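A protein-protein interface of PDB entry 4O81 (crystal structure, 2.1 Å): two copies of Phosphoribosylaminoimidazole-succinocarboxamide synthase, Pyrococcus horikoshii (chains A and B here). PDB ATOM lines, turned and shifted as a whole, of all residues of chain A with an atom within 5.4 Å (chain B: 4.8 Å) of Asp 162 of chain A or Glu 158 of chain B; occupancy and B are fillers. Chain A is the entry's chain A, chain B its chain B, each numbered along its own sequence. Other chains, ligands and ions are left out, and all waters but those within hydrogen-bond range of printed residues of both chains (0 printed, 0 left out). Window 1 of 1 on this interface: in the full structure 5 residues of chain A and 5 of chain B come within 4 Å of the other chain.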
ATOM      1  N   ASN A 157     -13.014 -27.890   2.591  1.00  0.00           N
ATOM      2  CA  ASN A 157     -13.097 -27.700   1.142  1.00  0.00           C
ATOM      3  C   ASN A 157     -13.735 -26.364   0.764  1.00  0.00           C
ATOM      4  O   ASN A 157     -13.199 -25.632  -0.079  1.00  0.00           O
ATOM      5  CB  ASN A 157     -13.874 -28.831   0.467  1.00  0.00           C
ATOM      6  CG  ASN A 157     -13.971 -28.647  -1.039  1.00  0.00           C
ATOM      7  OD1 ASN A 157     -12.945 -28.551  -1.719  1.00  0.00           O
ATOM      8  ND2 ASN A 157     -15.207 -28.610  -1.576  1.00  0.00           N
ATOM      9  N   GLU A 158     -14.871 -26.053   1.383  1.00  0.00           N
ATOM     10  CA  GLU A 158     -15.628 -24.888   0.974  1.00  0.00           C
ATOM     11  C   GLU A 158     -14.865 -23.603   1.291  1.00  0.00           C
ATOM     12  O   GLU A 158     -14.847 -22.663   0.478  1.00  0.00           O
ATOM     13  CB  GLU A 158     -17.035 -24.878   1.598  1.00  0.00           C
ATOM     14  CG  GLU A 158     -18.063 -24.107   0.764  1.00  0.00           C
ATOM     15  CD  GLU A 158     -18.278 -24.690  -0.629  1.00  0.00           C
ATOM     16  OE1 GLU A 158     -18.117 -25.924  -0.825  1.00  0.00           O
ATOM     17  OE2 GLU A 158     -18.601 -23.911  -1.544  1.00  0.00           O
ATOM     18  N   ILE A 159     -14.210 -23.578   2.448  1.00  0.00           N
ATOM     19  CA  ILE A 159     -13.456 -22.390   2.873  1.00  0.00           C
ATOM     20  C   ILE A 159     -12.261 -22.165   1.930  1.00  0.00           C
ATOM     21  O   ILE A 159     -12.035 -21.050   1.442  1.00  0.00           O
ATOM     22  CB  ILE A 159     -12.986 -22.513   4.336  1.00  0.00           C
ATOM     23  CG1 ILE A 159     -14.192 -22.589   5.276  1.00  0.00           C
ATOM     24  CG2 ILE A 159     -12.075 -21.354   4.728  1.00  0.00           C
ATOM     25  CD1 ILE A 159     -13.882 -23.262   6.604  1.00  0.00           C
ATOM     26  N   LEU A 160     -11.519 -23.233   1.659  1.00  0.00           N
ATOM     27  CA  LEU A 160     -10.336 -23.123   0.789  1.00  0.00           C
ATOM     28  C   LEU A 160     -10.727 -22.800  -0.650  1.00  0.00           C
ATOM     29  O   LEU A 160     -10.140 -21.909  -1.268  1.00  0.00           O
ATOM     30  CB  LEU A 160      -9.439 -24.368   0.887  1.00  0.00           C
ATOM     31  CG  LEU A 160      -8.779 -24.655   2.256  1.00  0.00           C
ATOM     32  CD1 LEU A 160      -7.817 -25.815   2.162  1.00  0.00           C
ATOM     33  CD2 LEU A 160      -8.070 -23.461   2.879  1.00  0.00           C
ATOM     34  N   LYS A 161     -11.747 -23.493  -1.162  1.00  0.00           N
ATOM     35  CA  LYS A 161     -12.254 -23.256  -2.506  1.00  0.00           C
ATOM     36  C   LYS A 161     -12.687 -21.799  -2.718  1.00  0.00           C
ATOM     37  O   LYS A 161     -12.282 -21.172  -3.707  1.00  0.00           O
ATOM     38  CB  LYS A 161     -13.441 -24.167  -2.814  1.00  0.00           C
ATOM     39  CG  LYS A 161     -13.938 -24.026  -4.246  1.00  0.00           C
ATOM     40  CD  LYS A 161     -15.173 -24.887  -4.505  1.00  0.00           C
ATOM     41  CE  LYS A 161     -16.363 -24.378  -3.700  1.00  0.00           C
ATOM     42  NZ  LYS A 161     -17.658 -24.848  -4.247  1.00  0.00           N
ATOM     43  N   ASP A 162     -13.505 -21.281  -1.797  1.00  0.00           N
ATOM     44  CA  ASP A 162     -14.035 -19.926  -1.919  1.00  0.00           C
ATOM     45  C   ASP A 162     -12.928 -18.872  -1.775  1.00  0.00           C
ATOM     46  O   ASP A 162     -12.894 -17.893  -2.502  1.00  0.00           O
ATOM     47  CB  ASP A 162     -15.144 -19.680  -0.895  1.00  0.00           C
ATOM     48  CG  ASP A 162     -16.386 -20.539  -1.150  1.00  0.00           C
ATOM     49  OD1 ASP A 162     -16.470 -21.217  -2.207  1.00  0.00           O
ATOM     50  OD2 ASP A 162     -17.274 -20.563  -0.273  1.00  0.00           O
ATOM     51  N   TYR A 163     -12.040 -19.090  -0.817  1.00  0.00           N
ATOM     52  CA  TYR A 163     -10.895 -18.202  -0.587  1.00  0.00           C
ATOM     53  C   TYR A 163     -10.028 -18.076  -1.845  1.00  0.00           C
ATOM     54  O   TYR A 163      -9.709 -16.967  -2.292  1.00  0.00           O
ATOM     55  CB  TYR A 163     -10.074 -18.743   0.586  1.00  0.00           C
ATOM     56  CG  TYR A 163      -8.835 -17.946   0.909  1.00  0.00           C
ATOM     57  CD1 TYR A 163      -8.918 -16.744   1.610  1.00  0.00           C
ATOM     58  CD2 TYR A 163      -7.582 -18.404   0.527  1.00  0.00           C
ATOM     59  CE1 TYR A 163      -7.777 -16.010   1.917  1.00  0.00           C
ATOM     60  CE2 TYR A 163      -6.435 -17.679   0.817  1.00  0.00           C
ATOM     61  CZ  TYR A 163      -6.541 -16.482   1.511  1.00  0.00           C
ATOM     62  OH  TYR A 163      -5.397 -15.773   1.796  1.00  0.00           O
ATOM     63  N   LEU A 164      -9.701 -19.225  -2.430  1.00  0.00           N
ATOM     64  CA  LEU A 164      -8.854 -19.292  -3.616  1.00  0.00           C
ATOM     65  C   LEU A 164      -9.561 -18.819  -4.881  1.00  0.00           C
ATOM     66  O   LEU A 164      -8.936 -18.212  -5.765  1.00  0.00           O
ATOM     67  CB  LEU A 164      -8.290 -20.710  -3.805  1.00  0.00           C
ATOM     68  CG  LEU A 164      -7.355 -21.203  -2.701  1.00  0.00           C
ATOM     69  CD1 LEU A 164      -7.135 -22.700  -2.848  1.00  0.00           C
ATOM     70  CD2 LEU A 164      -6.022 -20.454  -2.729  1.00  0.00           C
ATOM     71  N   ALA A 165     -10.862 -19.086  -4.970  1.00  0.00           N
ATOM     72  CA  ALA A 165     -11.656 -18.659  -6.128  1.00  0.00           C
ATOM     73  C   ALA A 165     -11.637 -17.139  -6.294  1.00  0.00           C
ATOM     74  O   ALA A 165     -11.595 -16.643  -7.410  1.00  0.00           O
ATOM     75  CB  ALA A 165     -13.095 -19.176  -6.043  1.00  0.00           C
ATOM     76  N   LYS A 166     -11.678 -16.404  -5.182  1.00  0.00           N
ATOM     77  CA  LYS A 166     -11.617 -14.938  -5.227  1.00  0.00           C
ATOM     78  C   LYS A 166     -10.259 -14.423  -5.702  1.00  0.00           C
ATOM     79  O   LYS A 166     -10.131 -13.257  -6.072  1.00  0.00           O
ATOM     80  CB  LYS A 166     -11.905 -14.338  -3.856  1.00  0.00           C
ATOM     81  CG  LYS A 166     -13.306 -14.554  -3.329  1.00  0.00           C
ATOM     82  CD  LYS A 166     -13.226 -14.641  -1.815  1.00  0.00           C
ATOM     83  CE  LYS A 166     -14.588 -14.742  -1.173  1.00  0.00           C
ATOM     84  NZ  LYS A 166     -15.098 -13.381  -0.844  1.00  0.00           N
ATOM     85  N   PRO B 115     -23.598 -19.991   7.279  1.00  0.00           N
ATOM     86  CA  PRO B 115     -24.762 -19.173   6.919  1.00  0.00           C
ATOM     87  C   PRO B 115     -25.898 -19.349   7.922  1.00  0.00           C
ATOM     88  O   PRO B 115     -26.071 -20.439   8.456  1.00  0.00           O
ATOM     89  CB  PRO B 115     -25.183 -19.711   5.543  1.00  0.00           C
ATOM     90  CG  PRO B 115     -24.122 -20.648   5.109  1.00  0.00           C
ATOM     91  CD  PRO B 115     -23.352 -21.080   6.318  1.00  0.00           C
ATOM     92  N   LEU B 154     -30.252 -22.847   1.489  1.00  0.00           N
ATOM     93  CA  LEU B 154     -28.811 -22.914   1.730  1.00  0.00           C
ATOM     94  C   LEU B 154     -28.045 -23.283   0.459  1.00  0.00           C
ATOM     95  O   LEU B 154     -26.945 -22.780   0.229  1.00  0.00           O
ATOM     96  CB  LEU B 154     -28.460 -23.861   2.892  1.00  0.00           C
ATOM     97  CG  LEU B 154     -28.799 -23.368   4.299  1.00  0.00           C
ATOM     98  CD1 LEU B 154     -28.770 -24.525   5.289  1.00  0.00           C
ATOM     99  CD2 LEU B 154     -27.850 -22.264   4.726  1.00  0.00           C
ATOM    100  N   LYS B 155     -28.637 -24.146  -0.365  1.00  0.00           N
ATOM    101  CA  LYS B 155     -28.088 -24.454  -1.681  1.00  0.00           C
ATOM    102  C   LYS B 155     -28.023 -23.211  -2.567  1.00  0.00           C
ATOM    103  O   LYS B 155     -26.986 -22.921  -3.167  1.00  0.00           O
ATOM    104  CB  LYS B 155     -28.938 -25.502  -2.379  1.00  0.00           C
ATOM    105  CG  LYS B 155     -28.598 -26.935  -2.024  1.00  0.00           C
ATOM    106  CD  LYS B 155     -28.929 -27.837  -3.201  1.00  0.00           C
ATOM    107  CE  LYS B 155     -28.016 -27.511  -4.377  1.00  0.00           C
ATOM    108  NZ  LYS B 155     -28.525 -27.979  -5.699  1.00  0.00           N
ATOM    109  N   VAL B 156     -29.145 -22.492  -2.633  1.00  0.00           N
ATOM    110  CA  VAL B 156     -29.244 -21.248  -3.375  1.00  0.00           C
ATOM    111  C   VAL B 156     -28.197 -20.262  -2.875  1.00  0.00           C
ATOM    112  O   VAL B 156     -27.511 -19.625  -3.677  1.00  0.00           O
ATOM    113  CB  VAL B 156     -30.652 -20.610  -3.276  1.00  0.00           C
ATOM    114  CG1 VAL B 156     -30.634 -19.164  -3.809  1.00  0.00           C
ATOM    115  CG2 VAL B 156     -31.699 -21.453  -4.012  1.00  0.00           C
ATOM    116  N   ASN B 157     -28.088 -20.123  -1.549  1.00  0.00           N
ATOM    117  CA  ASN B 157     -27.082 -19.263  -0.972  1.00  0.00           C
ATOM    118  C   ASN B 157     -25.688 -19.563  -1.517  1.00  0.00           C
ATOM    119  O   ASN B 157     -24.954 -18.654  -1.900  1.00  0.00           O
ATOM    120  CB  ASN B 157     -27.048 -19.396   0.544  1.00  0.00           C
ATOM    121  CG  ASN B 157     -26.024 -18.470   1.184  1.00  0.00           C
ATOM    122  OD1 ASN B 157     -26.098 -17.243   1.026  1.00  0.00           O
ATOM    123  ND2 ASN B 157     -25.068 -19.052   1.920  1.00  0.00           N
ATOM    124  N   GLU B 158     -25.323 -20.844  -1.544  1.00  0.00           N
ATOM    125  CA  GLU B 158     -23.954 -21.174  -1.879  1.00  0.00           C
ATOM    126  C   GLU B 158     -23.625 -20.855  -3.334  1.00  0.00           C
ATOM    127  O   GLU B 158     -22.554 -20.332  -3.613  1.00  0.00           O
ATOM    128  CB  GLU B 158     -23.581 -22.614  -1.537  1.00  0.00           C
ATOM    129  CG  GLU B 158     -22.083 -22.746  -1.247  1.00  0.00           C
ATOM    130  CD  GLU B 158     -21.628 -21.970  -0.014  1.00  0.00           C
ATOM    131  OE1 GLU B 158     -22.453 -21.649   0.876  1.00  0.00           O
ATOM    132  OE2 GLU B 158     -20.430 -21.647   0.085  1.00  0.00           O
ATOM    133  N   ILE B 159     -24.565 -21.150  -4.225  1.00  0.00           N
ATOM    134  CA  ILE B 159     -24.418 -20.838  -5.654  1.00  0.00           C
ATOM    135  C   ILE B 159     -24.335 -19.327  -5.907  1.00  0.00           C
ATOM    136  O   ILE B 159     -23.450 -18.857  -6.628  1.00  0.00           O
ATOM    137  CB  ILE B 159     -25.589 -21.431  -6.468  1.00  0.00           C
ATOM    138  CG1 ILE B 159     -25.604 -22.962  -6.324  1.00  0.00           C
ATOM    139  CG2 ILE B 159     -25.505 -20.995  -7.936  1.00  0.00           C
ATOM    140  CD1 ILE B 159     -26.928 -23.616  -6.633  1.00  0.00           C
ATOM    141  N   LEU B 160     -25.265 -18.571  -5.333  1.00  0.00           N
ATOM    142  CA  LEU B 160     -25.254 -17.137  -5.524  1.00  0.00           C
ATOM    143  C   LEU B 160     -23.994 -16.508  -4.914  1.00  0.00           C
ATOM    144  O   LEU B 160     -23.338 -15.707  -5.561  1.00  0.00           O
ATOM    145  CB  LEU B 160     -26.548 -16.492  -4.997  1.00  0.00           C
ATOM    146  CG  LEU B 160     -27.882 -16.821  -5.700  1.00  0.00           C
ATOM    147  CD1 LEU B 160     -29.001 -15.938  -5.159  1.00  0.00           C
ATOM    148  CD2 LEU B 160     -27.817 -16.690  -7.220  1.00  0.00           C
ATOM    149  N   LYS B 161     -23.632 -16.914  -3.695  1.00  0.00           N
ATOM    150  CA  LYS B 161     -22.483 -16.341  -2.998  1.00  0.00           C
ATOM    151  C   LYS B 161     -21.189 -16.554  -3.771  1.00  0.00           C
ATOM    152  O   LYS B 161     -20.375 -15.624  -3.899  1.00  0.00           O
ATOM    153  CB  LYS B 161     -22.336 -16.938  -1.594  1.00  0.00           C
ATOM    154  CG  LYS B 161     -21.141 -16.408  -0.813  1.00  0.00           C
ATOM    155  CD  LYS B 161     -20.916 -17.147   0.502  1.00  0.00           C
ATOM    156  CE  LYS B 161     -20.534 -18.593   0.267  1.00  0.00           C
ATOM    157  NZ  LYS B 161     -19.939 -19.207   1.496  1.00  0.00           N
ATOM    158  N   ASP B 162     -21.007 -17.779  -4.262  1.00  0.00           N
ATOM    159  CA  ASP B 162     -19.770 -18.141  -4.955  1.00  0.00           C
ATOM    160  C   ASP B 162     -19.654 -17.433  -6.297  1.00  0.00           C
ATOM    161  O   ASP B 162     -18.578 -16.952  -6.645  1.00  0.00           O
ATOM    162  CB  ASP B 162     -19.682 -19.656  -5.128  1.00  0.00           C
ATOM    163  CG  ASP B 162     -19.478 -20.387  -3.797  1.00  0.00           C
ATOM    164  OD1 ASP B 162     -19.273 -19.728  -2.746  1.00  0.00           O
ATOM    165  OD2 ASP B 162     -19.494 -21.627  -3.802  1.00  0.00           O
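Of the 10 printed residues of chain B, 3 touch a printed residue of chain A. Among the printed residues, 6 pairs touch across the chains. Among the printed residues, Asp or Glu carboxylates within 4 Å of a Lys or Arg side-chain nitrogen of the other chain: Lys 161 of chain A with Asp 162 of chain B (3.7 Å) and Asp 162 of chain A with Lys 161 of chain B (3.5 Å).
Printed residues of chain B within 4 Å of Glu 158 of chain A: Glu 158 (3.3 Å) and Asp 162 (3.3 Å). Of the printed residues of chain B, Lys 161 of chain A touches Asp 162. Asp 162 of chain A touches just these residues of chain B: Glu 158 (3.4 Å), Lys 161 (3.5 Å) and Asp 162 (3.2 Å). Tyr 163 of chain A touches none of the printed residues of chain B. Printed residues of chain A within 4 Å of Glu 158 of chain B: Glu 158 (3.3 Å) and Asp 162 (3.4 Å). Of the printed residues of chain A, Lys 161 of chain B touches Asp 162. Of the printed residues of chain A, Asp 162 of chain B touches Glu 158, Lys 161 and Asp 162.
Glu 158 of chain A touches its own counterpart, Glu 158 of chain B. Glu 158 of chain A touches Asp 162 of chain B, and with the chains exchanged Asp 162 of chain A touches Glu 158 of chain B. Lys 161 of chain A touches Asp 162 of chain B, and with the chains exchanged Asp 162 of chain A touches Lys 161 of chain B. Asp 162 of chain A touches its own counterpart, Asp 162 of chain B. Positions printed for both chains: 157, 158, 159, 160, 161 and 162.
The side-chain carboxylate (OE1) of Glu 158 of chain A is in salt-bridge range of the side-chain amino group (NZ) of Lys 161 of chain A (3.6 Å). The side-chain carboxylate of Glu 158 of chain B lies within salt-bridge range of the side-chain amino group of Lys 161 of chain B (3.6 Å).
The side-chain carboxylate (OD2) of Asp 162 of chain B sits close to the side-chain amino group (NZ) of Lys 161 of chain A (3.7 Å). OD2 of Asp 162 of chain A sits close to NZ of Lys 161 of chain B, 3.5 Å away. The side-chain carboxylate of Glu 158 of chain B sits close to the side-chain carboxylate of Glu 158 of chain A. The side-chain carboxylate of Glu 158 of chain A lies close to the side-chain carboxylate of Asp 162 of chain B. OD2 of Asp 162 of chain A sits close to OE2 of Glu 158 of chain B. The side-chain carboxylate (OD1) of Asp 162 of chain B sits close to the side-chain carboxylate (OD1) of Asp 162 of chain A, at 3.2 Å.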
